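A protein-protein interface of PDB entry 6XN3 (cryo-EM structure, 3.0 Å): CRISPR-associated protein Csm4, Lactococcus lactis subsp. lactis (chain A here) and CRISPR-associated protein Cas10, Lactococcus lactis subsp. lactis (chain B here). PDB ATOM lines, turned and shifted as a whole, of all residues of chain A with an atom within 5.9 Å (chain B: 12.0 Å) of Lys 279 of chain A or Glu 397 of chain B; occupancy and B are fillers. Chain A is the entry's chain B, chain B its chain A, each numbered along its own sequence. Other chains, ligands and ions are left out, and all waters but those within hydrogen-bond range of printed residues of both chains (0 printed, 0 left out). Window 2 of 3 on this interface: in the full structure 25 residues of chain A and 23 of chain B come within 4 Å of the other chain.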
ATOM      1  N   TYR A 246      28.324 -12.959  -7.255  1.00  0.00           N
ATOM      2  CA  TYR A 246      27.053 -13.097  -7.957  1.00  0.00           C
ATOM      3  C   TYR A 246      25.969 -13.419  -6.940  1.00  0.00           C
ATOM      4  O   TYR A 246      25.707 -14.589  -6.656  1.00  0.00           O
ATOM      5  CB  TYR A 246      27.135 -14.182  -9.024  1.00  0.00           C
ATOM      6  CG  TYR A 246      26.012 -14.196 -10.037  1.00  0.00           C
ATOM      7  CD1 TYR A 246      24.801 -14.812  -9.761  1.00  0.00           C
ATOM      8  CD2 TYR A 246      26.181 -13.623 -11.285  1.00  0.00           C
ATOM      9  CE1 TYR A 246      23.788 -14.832 -10.686  1.00  0.00           C
ATOM     10  CE2 TYR A 246      25.175 -13.645 -12.220  1.00  0.00           C
ATOM     11  CZ  TYR A 246      23.982 -14.248 -11.913  1.00  0.00           C
ATOM     12  OH  TYR A 246      22.972 -14.267 -12.844  1.00  0.00           O
ATOM     13  N   ALA A 247      25.367 -12.373  -6.381  1.00  0.00           N
ATOM     14  CA  ALA A 247      24.026 -12.393  -5.796  1.00  0.00           C
ATOM     15  C   ALA A 247      23.868 -13.336  -4.606  1.00  0.00           C
ATOM     16  O   ALA A 247      22.949 -14.157  -4.599  1.00  0.00           O
ATOM     17  CB  ALA A 247      22.977 -12.734  -6.860  1.00  0.00           C
ATOM     18  N   VAL A 251      23.231 -19.418  -7.289  1.00  0.00           N
ATOM     19  CA  VAL A 251      22.231 -19.304  -8.335  1.00  0.00           C
ATOM     20  C   VAL A 251      22.675 -20.130  -9.530  1.00  0.00           C
ATOM     21  O   VAL A 251      23.847 -20.103  -9.915  1.00  0.00           O
ATOM     22  CB  VAL A 251      22.037 -17.827  -8.707  1.00  0.00           C
ATOM     23  CG1 VAL A 251      20.982 -17.667  -9.775  1.00  0.00           C
ATOM     24  CG2 VAL A 251      21.684 -17.031  -7.474  1.00  0.00           C
ATOM     25  N   LYS A 252      21.744 -20.874 -10.120  1.00  0.00           N
ATOM     26  CA  LYS A 252      22.058 -21.673 -11.293  1.00  0.00           C
ATOM     27  C   LYS A 252      22.298 -20.780 -12.507  1.00  0.00           C
ATOM     28  O   LYS A 252      22.033 -19.577 -12.496  1.00  0.00           O
ATOM     29  CB  LYS A 252      20.929 -22.656 -11.597  1.00  0.00           C
ATOM     30  CG  LYS A 252      20.845 -23.819 -10.638  1.00  0.00           C
ATOM     31  CD  LYS A 252      20.234 -25.037 -11.286  1.00  0.00           C
ATOM     32  CE  LYS A 252      21.247 -25.784 -12.116  1.00  0.00           C
ATOM     33  NZ  LYS A 252      20.590 -26.680 -13.095  1.00  0.00           N
ATOM     34  N   LYS A 253      22.821 -21.384 -13.562  1.00  0.00           N
ATOM     35  CA  LYS A 253      23.047 -20.664 -14.801  1.00  0.00           C
ATOM     36  C   LYS A 253      21.898 -20.900 -15.767  1.00  0.00           C
ATOM     37  O   LYS A 253      21.164 -21.884 -15.671  1.00  0.00           O
ATOM     38  CB  LYS A 253      24.361 -21.090 -15.451  1.00  0.00           C
ATOM     39  CG  LYS A 253      25.582 -20.470 -14.830  1.00  0.00           C
ATOM     40  CD  LYS A 253      26.778 -20.603 -15.736  1.00  0.00           C
ATOM     41  CE  LYS A 253      27.417 -21.961 -15.612  1.00  0.00           C
ATOM     42  NZ  LYS A 253      28.122 -22.088 -14.318  1.00  0.00           N
ATOM     43  N   GLN A 254      21.746 -19.968 -16.700  1.00  0.00           N
ATOM     44  CA  GLN A 254      20.859 -20.153 -17.835  1.00  0.00           C
ATOM     45  C   GLN A 254      21.420 -21.274 -18.692  1.00  0.00           C
ATOM     46  O   GLN A 254      22.485 -21.108 -19.290  1.00  0.00           O
ATOM     47  CB  GLN A 254      20.760 -18.854 -18.627  1.00  0.00           C
ATOM     48  CG  GLN A 254      19.582 -18.743 -19.557  1.00  0.00           C
ATOM     49  CD  GLN A 254      19.278 -17.301 -19.885  1.00  0.00           C
ATOM     50  OE1 GLN A 254      19.042 -16.493 -18.991  1.00  0.00           O
ATOM     51  NE2 GLN A 254      19.290 -16.967 -21.168  1.00  0.00           N
ATOM     52  N   VAL A 276      25.098 -15.845 -19.832  1.00  0.00           N
ATOM     53  CA  VAL A 276      24.141 -16.789 -19.272  1.00  0.00           C
ATOM     54  C   VAL A 276      23.854 -16.426 -17.826  1.00  0.00           C
ATOM     55  O   VAL A 276      23.239 -17.202 -17.087  1.00  0.00           O
ATOM     56  CB  VAL A 276      24.656 -18.230 -19.375  1.00  0.00           C
ATOM     57  CG1 VAL A 276      24.813 -18.621 -20.813  1.00  0.00           C
ATOM     58  CG2 VAL A 276      25.969 -18.351 -18.661  1.00  0.00           C
ATOM     59  N   GLY A 277      24.304 -15.255 -17.410  1.00  0.00           N
ATOM     60  CA  GLY A 277      23.928 -14.739 -16.113  1.00  0.00           C
ATOM     61  C   GLY A 277      23.560 -13.280 -16.229  1.00  0.00           C
ATOM     62  O   GLY A 277      24.387 -12.459 -16.630  1.00  0.00           O
ATOM     63  N   LYS A 278      22.323 -12.938 -15.887  1.00  0.00           N
ATOM     64  CA  LYS A 278      21.858 -11.572 -16.072  1.00  0.00           C
ATOM     65  C   LYS A 278      21.118 -11.065 -14.848  1.00  0.00           C
ATOM     66  O   LYS A 278      20.269 -10.177 -14.958  1.00  0.00           O
ATOM     67  CB  LYS A 278      20.959 -11.466 -17.299  1.00  0.00           C
ATOM     68  CG  LYS A 278      19.875 -12.524 -17.351  1.00  0.00           C
ATOM     69  CD  LYS A 278      19.156 -12.510 -18.686  1.00  0.00           C
ATOM     70  CE  LYS A 278      19.867 -13.355 -19.714  1.00  0.00           C
ATOM     71  NZ  LYS A 278      18.995 -13.588 -20.893  1.00  0.00           N
ATOM     72  N   LYS A 279      21.414 -11.623 -13.677  1.00  0.00           N
ATOM     73  CA  LYS A 279      20.733 -11.205 -12.458  1.00  0.00           C
ATOM     74  C   LYS A 279      21.658 -10.897 -11.295  1.00  0.00           C
ATOM     75  O   LYS A 279      21.200 -10.288 -10.324  1.00  0.00           O
ATOM     76  CB  LYS A 279      19.726 -12.271 -12.013  1.00  0.00           C
ATOM     77  CG  LYS A 279      18.531 -12.439 -12.937  1.00  0.00           C
ATOM     78  CD  LYS A 279      17.550 -13.458 -12.387  1.00  0.00           C
ATOM     79  CE  LYS A 279      16.457 -13.763 -13.391  1.00  0.00           C
ATOM     80  NZ  LYS A 279      15.629 -12.559 -13.663  1.00  0.00           N
ATOM     81  N   GLY A 280      22.927 -11.277 -11.337  1.00  0.00           N
ATOM     82  CA  GLY A 280      23.826 -11.021 -10.237  1.00  0.00           C
ATOM     83  C   GLY A 280      24.446  -9.642 -10.316  1.00  0.00           C
ATOM     84  O   GLY A 280      23.940  -8.725 -10.966  1.00  0.00           O
ATOM     85  N   ASN A 281      25.574  -9.499  -9.625  1.00  0.00           N
ATOM     86  CA  ASN A 281      26.278  -8.228  -9.594  1.00  0.00           C
ATOM     87  C   ASN A 281      27.347  -8.110 -10.671  1.00  0.00           C
ATOM     88  O   ASN A 281      27.988  -7.060 -10.772  1.00  0.00           O
ATOM     89  CB  ASN A 281      26.901  -8.022  -8.218  1.00  0.00           C
ATOM     90  CG  ASN A 281      25.887  -7.574  -7.194  1.00  0.00           C
ATOM     91  OD1 ASN A 281      24.691  -7.528  -7.473  1.00  0.00           O
ATOM     92  ND2 ASN A 281      26.357  -7.234  -6.003  1.00  0.00           N
ATOM     93  N   LYS B 340      14.153 -32.426 -21.999  1.00  0.00           N
ATOM     94  CA  LYS B 340      14.686 -31.348 -22.831  1.00  0.00           C
ATOM     95  C   LYS B 340      15.551 -31.809 -23.999  1.00  0.00           C
ATOM     96  O   LYS B 340      15.301 -31.416 -25.140  1.00  0.00           O
ATOM     97  CB  LYS B 340      15.490 -30.390 -21.960  1.00  0.00           C
ATOM     98  CG  LYS B 340      14.689 -29.720 -20.861  1.00  0.00           C
ATOM     99  CD  LYS B 340      13.795 -28.627 -21.401  1.00  0.00           C
ATOM    100  CE  LYS B 340      13.241 -27.788 -20.268  1.00  0.00           C
ATOM    101  NZ  LYS B 340      12.444 -26.634 -20.762  1.00  0.00           N
ATOM    102  N   LEU B 391      14.411 -23.784 -27.444  1.00  0.00           N
ATOM    103  CA  LEU B 391      15.024 -24.549 -26.371  1.00  0.00           C
ATOM    104  C   LEU B 391      16.113 -23.760 -25.660  1.00  0.00           C
ATOM    105  O   LEU B 391      16.388 -24.001 -24.480  1.00  0.00           O
ATOM    106  CB  LEU B 391      15.534 -25.853 -26.976  1.00  0.00           C
ATOM    107  CG  LEU B 391      16.157 -27.004 -26.223  1.00  0.00           C
ATOM    108  CD1 LEU B 391      15.850 -28.277 -26.910  1.00  0.00           C
ATOM    109  CD2 LEU B 391      17.574 -26.787 -26.466  1.00  0.00           C
ATOM    110  N   ASN B 392      16.752 -22.826 -26.355  1.00  0.00           N
ATOM    111  CA  ASN B 392      17.687 -21.936 -25.674  1.00  0.00           C
ATOM    112  C   ASN B 392      16.980 -20.735 -25.061  1.00  0.00           C
ATOM    113  O   ASN B 392      17.431 -20.207 -24.043  1.00  0.00           O
ATOM    114  CB  ASN B 392      18.776 -21.473 -26.634  1.00  0.00           C
ATOM    115  CG  ASN B 392      19.955 -22.404 -26.657  1.00  0.00           C
ATOM    116  OD1 ASN B 392      20.509 -22.745 -25.617  1.00  0.00           O
ATOM    117  ND2 ASN B 392      20.339 -22.840 -27.843  1.00  0.00           N
ATOM    118  N   HIS B 393      15.881 -20.284 -25.666  1.00  0.00           N
ATOM    119  CA  HIS B 393      15.197 -19.109 -25.141  1.00  0.00           C
ATOM    120  C   HIS B 393      14.400 -19.401 -23.880  1.00  0.00           C
ATOM    121  O   HIS B 393      14.179 -18.486 -23.083  1.00  0.00           O
ATOM    122  CB  HIS B 393      14.280 -18.515 -26.204  1.00  0.00           C
ATOM    123  CG  HIS B 393      13.838 -17.118 -25.906  1.00  0.00           C
ATOM    124  ND1 HIS B 393      12.899 -16.823 -24.942  1.00  0.00           N
ATOM    125  CD2 HIS B 393      14.217 -15.932 -26.438  1.00  0.00           C
ATOM    126  CE1 HIS B 393      12.712 -15.516 -24.897  1.00  0.00           C
ATOM    127  NE2 HIS B 393      13.499 -14.953 -25.796  1.00  0.00           N
ATOM    128  N   GLN B 394      13.967 -20.643 -23.668  1.00  0.00           N
ATOM    129  CA  GLN B 394      13.222 -20.971 -22.458  1.00  0.00           C
ATOM    130  C   GLN B 394      14.112 -21.191 -21.239  1.00  0.00           C
ATOM    131  O   GLN B 394      13.633 -21.715 -20.230  1.00  0.00           O
ATOM    132  CB  GLN B 394      12.350 -22.211 -22.681  1.00  0.00           C
ATOM    133  CG  GLN B 394      11.257 -22.029 -23.719  1.00  0.00           C
ATOM    134  CD  GLN B 394       9.915 -21.669 -23.117  1.00  0.00           C
ATOM    135  OE1 GLN B 394       9.839 -20.996 -22.093  1.00  0.00           O
ATOM    136  NE2 GLN B 394       8.842 -22.116 -23.759  1.00  0.00           N
ATOM    137  N   GLY B 395      15.386 -20.816 -21.303  1.00  0.00           N
ATOM    138  CA  GLY B 395      16.263 -20.995 -20.160  1.00  0.00           C
ATOM    139  C   GLY B 395      16.073 -19.881 -19.150  1.00  0.00           C
ATOM    140  O   GLY B 395      15.928 -18.708 -19.511  1.00  0.00           O
ATOM    141  N   THR B 396      16.070 -20.249 -17.874  1.00  0.00           N
ATOM    142  CA  THR B 396      15.986 -19.290 -16.786  1.00  0.00           C
ATOM    143  C   THR B 396      16.806 -19.822 -15.625  1.00  0.00           C
ATOM    144  O   THR B 396      17.138 -21.008 -15.569  1.00  0.00           O
ATOM    145  CB  THR B 396      14.538 -19.033 -16.356  1.00  0.00           C
ATOM    146  OG1 THR B 396      14.506 -17.980 -15.385  1.00  0.00           O
ATOM    147  CG2 THR B 396      13.918 -20.288 -15.772  1.00  0.00           C
ATOM    148  N   GLU B 397      17.144 -18.932 -14.705  1.00  0.00           N
ATOM    149  CA  GLU B 397      17.994 -19.276 -13.581  1.00  0.00           C
ATOM    150  C   GLU B 397      17.176 -19.298 -12.298  1.00  0.00           C
ATOM    151  O   GLU B 397      16.288 -18.465 -12.098  1.00  0.00           O
ATOM    152  CB  GLU B 397      19.180 -18.309 -13.492  1.00  0.00           C
ATOM    153  CG  GLU B 397      18.841 -16.872 -13.180  1.00  0.00           C
ATOM    154  CD  GLU B 397      20.023 -15.953 -13.377  1.00  0.00           C
ATOM    155  OE1 GLU B 397      20.273 -15.548 -14.530  1.00  0.00           O
ATOM    156  OE2 GLU B 397      20.704 -15.633 -12.385  1.00  0.00           O
ATOM    157  N   ASN B 398      17.433 -20.300 -11.460  1.00  0.00           N
ATOM    158  CA  ASN B 398      16.714 -20.463 -10.208  1.00  0.00           C
ATOM    159  C   ASN B 398      17.669 -20.988  -9.150  1.00  0.00           C
ATOM    160  O   ASN B 398      18.758 -21.472  -9.454  1.00  0.00           O
ATOM    161  CB  ASN B 398      15.527 -21.422 -10.335  1.00  0.00           C
ATOM    162  CG  ASN B 398      14.471 -20.922 -11.296  1.00  0.00           C
ATOM    163  OD1 ASN B 398      14.240 -21.527 -12.340  1.00  0.00           O
ATOM    164  ND2 ASN B 398      13.825 -19.814 -10.950  1.00  0.00           N
ATOM    165  N   ALA B 399      17.237 -20.898  -7.896  1.00  0.00           N
ATOM    166  CA  ALA B 399      18.039 -21.332  -6.762  1.00  0.00           C
ATOM    167  C   ALA B 399      17.708 -22.754  -6.327  1.00  0.00           C
ATOM    168  O   ALA B 399      18.202 -23.217  -5.295  1.00  0.00           O
ATOM    169  CB  ALA B 399      17.863 -20.362  -5.596  1.00  0.00           C
ATOM    170  N   ARG B 400      16.882 -23.460  -7.092  1.00  0.00           N
ATOM    171  CA  ARG B 400      16.486 -24.807  -6.718  1.00  0.00           C
ATOM    172  C   ARG B 400      16.668 -25.733  -7.906  1.00  0.00           C
ATOM    173  O   ARG B 400      16.616 -25.310  -9.061  1.00  0.00           O
ATOM    174  CB  ARG B 400      15.033 -24.863  -6.242  1.00  0.00           C
ATOM    175  CG  ARG B 400      14.775 -24.157  -4.932  1.00  0.00           C
ATOM    176  CD  ARG B 400      13.444 -24.577  -4.334  1.00  0.00           C
ATOM    177  NE  ARG B 400      12.314 -24.266  -5.201  1.00  0.00           N
ATOM    178  CZ  ARG B 400      11.508 -25.177  -5.735  1.00  0.00           C
ATOM    179  NH1 ARG B 400      11.706 -26.465  -5.491  1.00  0.00           N
ATOM    180  NH2 ARG B 400      10.501 -24.801  -6.509  1.00  0.00           N
ATOM    181  N   GLU B 401      16.886 -27.007  -7.608  1.00  0.00           N
ATOM    182  CA  GLU B 401      16.829 -28.036  -8.633  1.00  0.00           C
ATOM    183  C   GLU B 401      16.336 -29.301  -7.953  1.00  0.00           C
ATOM    184  O   GLU B 401      16.375 -29.416  -6.725  1.00  0.00           O
ATOM    185  CB  GLU B 401      18.188 -28.300  -9.272  1.00  0.00           C
ATOM    186  CG  GLU B 401      19.157 -28.944  -8.313  1.00  0.00           C
ATOM    187  CD  GLU B 401      20.573 -28.964  -8.811  1.00  0.00           C
ATOM    188  OE1 GLU B 401      20.867 -29.687  -9.778  1.00  0.00           O
ATOM    189  OE2 GLU B 401      21.417 -28.322  -8.176  1.00  0.00           O
ATOM    190  N   CYS B 402      15.848 -30.236  -8.754  1.00  0.00           N
ATOM    191  CA  CYS B 402      15.682 -31.576  -8.230  1.00  0.00           C
ATOM    192  C   CYS B 402      17.002 -32.327  -8.222  1.00  0.00           C
ATOM    193  O   CYS B 402      17.944 -31.997  -8.943  1.00  0.00           O
ATOM    194  CB  CYS B 402      14.665 -32.364  -9.028  1.00  0.00           C
ATOM    195  SG  CYS B 402      14.582 -34.056  -8.440  1.00  0.00           S
ATOM    196  N   LYS B 406      18.329 -33.146 -12.538  1.00  0.00           N
ATOM    197  CA  LYS B 406      18.917 -31.871 -12.139  1.00  0.00           C
ATOM    198  C   LYS B 406      18.408 -30.772 -13.059  1.00  0.00           C
ATOM    199  O   LYS B 406      19.051 -30.414 -14.047  1.00  0.00           O
ATOM    200  CB  LYS B 406      20.439 -31.945 -12.137  1.00  0.00           C
ATOM    201  CG  LYS B 406      20.977 -32.763 -10.984  1.00  0.00           C
ATOM    202  CD  LYS B 406      22.428 -32.469 -10.719  1.00  0.00           C
ATOM    203  CE  LYS B 406      22.758 -32.685  -9.265  1.00  0.00           C
ATOM    204  NZ  LYS B 406      22.254 -34.004  -8.813  1.00  0.00           N
ATOM    205  N   ARG B 407      17.241 -30.243 -12.720  1.00  0.00           N
ATOM    206  CA  ARG B 407      16.362 -29.553 -13.645  1.00  0.00           C
ATOM    207  C   ARG B 407      15.624 -28.440 -12.916  1.00  0.00           C
ATOM    208  O   ARG B 407      14.999 -28.649 -11.875  1.00  0.00           O
ATOM    209  CB  ARG B 407      15.385 -30.557 -14.257  1.00  0.00           C
ATOM    210  CG  ARG B 407      14.990 -30.294 -15.678  1.00  0.00           C
ATOM    211  CD  ARG B 407      14.095 -31.412 -16.158  1.00  0.00           C
ATOM    212  NE  ARG B 407      12.713 -31.223 -15.751  1.00  0.00           N
ATOM    213  CZ  ARG B 407      11.813 -30.580 -16.479  1.00  0.00           C
ATOM    214  NH1 ARG B 407      12.153 -30.060 -17.649  1.00  0.00           N
ATOM    215  NH2 ARG B 407      10.575 -30.458 -16.036  1.00  0.00           N
ATOM    216  N   SER B 408      15.681 -27.249 -13.494  1.00  0.00           N
ATOM    217  CA  SER B 408      15.368 -26.021 -12.780  1.00  0.00           C
ATOM    218  C   SER B 408      13.990 -25.502 -13.140  1.00  0.00           C
ATOM    219  O   SER B 408      13.704 -24.312 -12.995  1.00  0.00           O
ATOM    220  CB  SER B 408      16.423 -24.957 -13.060  1.00  0.00           C
ATOM    221  OG  SER B 408      16.001 -23.693 -12.587  1.00  0.00           O
ATOM    222  N   ASP B 409      13.110 -26.376 -13.609  1.00  0.00           N
ATOM    223  CA  ASP B 409      11.760 -25.948 -13.941  1.00  0.00           C
ATOM    224  C   ASP B 409      10.823 -27.122 -13.736  1.00  0.00           C
ATOM    225  O   ASP B 409      11.255 -28.277 -13.703  1.00  0.00           O
ATOM    226  CB  ASP B 409      11.659 -25.430 -15.375  1.00  0.00           C
ATOM    227  CG  ASP B 409      12.255 -26.384 -16.374  1.00  0.00           C
ATOM    228  OD1 ASP B 409      13.033 -27.265 -15.956  1.00  0.00           O
ATOM    229  OD2 ASP B 409      11.943 -26.261 -17.576  1.00  0.00           O
ATOM    230  N   LEU B 410       9.530 -26.799 -13.633  1.00  0.00           N
ATOM    231  CA  LEU B 410       8.456 -27.740 -13.306  1.00  0.00           C
ATOM    232  C   LEU B 410       8.748 -28.474 -12.000  1.00  0.00           C
ATOM    233  O   LEU B 410       8.687 -29.700 -11.931  1.00  0.00           O
ATOM    234  CB  LEU B 410       8.198 -28.726 -14.449  1.00  0.00           C
ATOM    235  CG  LEU B 410       7.660 -28.067 -15.715  1.00  0.00           C
ATOM    236  CD1 LEU B 410       7.561 -29.070 -16.842  1.00  0.00           C
ATOM    237  CD2 LEU B 410       6.313 -27.432 -15.442  1.00  0.00           C
ATOM    238  N   LEU B 411       9.079 -27.712 -10.966  1.00  0.00           N
ATOM    239  CA  LEU B 411       9.327 -28.237  -9.636  1.00  0.00           C
ATOM    240  C   LEU B 411       8.153 -27.891  -8.737  1.00  0.00           C
ATOM    241  O   LEU B 411       7.536 -26.833  -8.887  1.00  0.00           O
ATOM    242  CB  LEU B 411      10.612 -27.664  -9.056  1.00  0.00           C
ATOM    243  CG  LEU B 411      11.893 -28.367  -9.479  1.00  0.00           C
ATOM    244  CD1 LEU B 411      13.066 -27.419  -9.381  1.00  0.00           C
ATOM    245  CD2 LEU B 411      12.108 -29.574  -8.598  1.00  0.00           C
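The side-chain carboxylate (OE2) of Glu 397 of chain B is in hydrogen-bond range of the side-chain hydroxyl (OH) of Tyr 246 of chain A, at 2.7 Å.
O of Asn 398 of chain B lies within hydrogen-bond range of N of Lys 252 of chain A (3.1 Å).
The backbone NH (N) of Gln 254 of chain A sits at hydrogen-bond distance from the backbone carbonyl oxygen (O) of Val 276 of chain A (3.2 Å).
The side-chain amide oxygen of Asn 398 of chain B sits at hydrogen-bond distance from the side-chain hydroxyl of Ser 408 of chain B, 2.8 Å away.
The backbone NH (N) of Gly 280 of chain A lies close to the side-chain hydroxyl (OH) of Tyr 246 of chain A (3.3 Å).
The side-chain hydroxyl (OH) of Tyr 246 of chain A lies within hydrogen-bond range of the backbone NH (N) of Lys 278 of chain A (3.4 Å).
N of Lys 279 of chain A is in hydrogen-bond range of OH of Tyr 246 of chain A (3.2 Å).
The side-chain amide nitrogen of Gln 254 of chain A lies close to the side-chain amino group of Lys 278 of chain A, 3.4 Å away.
Of the 12 printed residues of chain A, 6 touch a printed residue of chain B.
Among the printed residues, 7 pairs touch across the chains.
Among the printed residues, no Asp or Glu carboxylate lies within 4 Å of a Lys or Arg side-chain nitrogen of the other chain.
Val 251 of chain A touches Glu 397 of chain B (CG1 to OE2, 3.3 Å).
Lys 252 of chain A touches Glu 397 of chain B.
Gln 254 of chain A touches Gly 395 of chain B.
Glu 397 of chain B touches Lys 278 of chain A (OE1 to N, 3.6 Å).
Lys 279 of chain A touches Glu 397 of chain B (CB to OE2, 3.5 Å).
Printed residues of chain B within 4 Å of Tyr 246 of chain A: Glu 397.
Ala 247 of chain A touches none of the printed residues of chain B.
Val 251 of chain A touches just one residue of chain B: Glu 397 (3.3 Å).
Lys 252 of chain A touches just these residues of chain B: Glu 397 (3.3 Å) and Asn 398 (3.1 Å).
Gln 254 of chain A touches just one residue of chain B: Gly 395 (3.7 Å).
No residue of chain B comes within 4 Å of Gly 277 of chain A.
Of the printed residues of chain B, Lys 279 of chain A touches Glu 397 (3.5 Å).
No residue of chain B comes within 4 Å of Gly 280 of chain A.
No residue of chain B comes within 4 Å of Asn 281 of chain A.
Of the printed residues of chain A, Gly 395 of chain B touches Gln 254.
Of the printed residues of chain A, Glu 397 of chain B touches Tyr 246 (2.7 Å), Val 251 (3.3 Å), Lys 252 (3.3 Å), Lys 278 (3.6 Å) and Lys 279 (3.5 Å).
Of the printed residues of chain A, Asn 398 of chain B touches Lys 252.
Arg 407 of chain B touches none of the printed residues of chain A.
The nearest residue of chain B that does not touch Lys 279 of chain A is Thr 396 of chain B (5.1 Å).
The nearest printed residue of chain A that does not touch Gly 395 of chain B is Lys 278 of chain A (6.1 Å).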
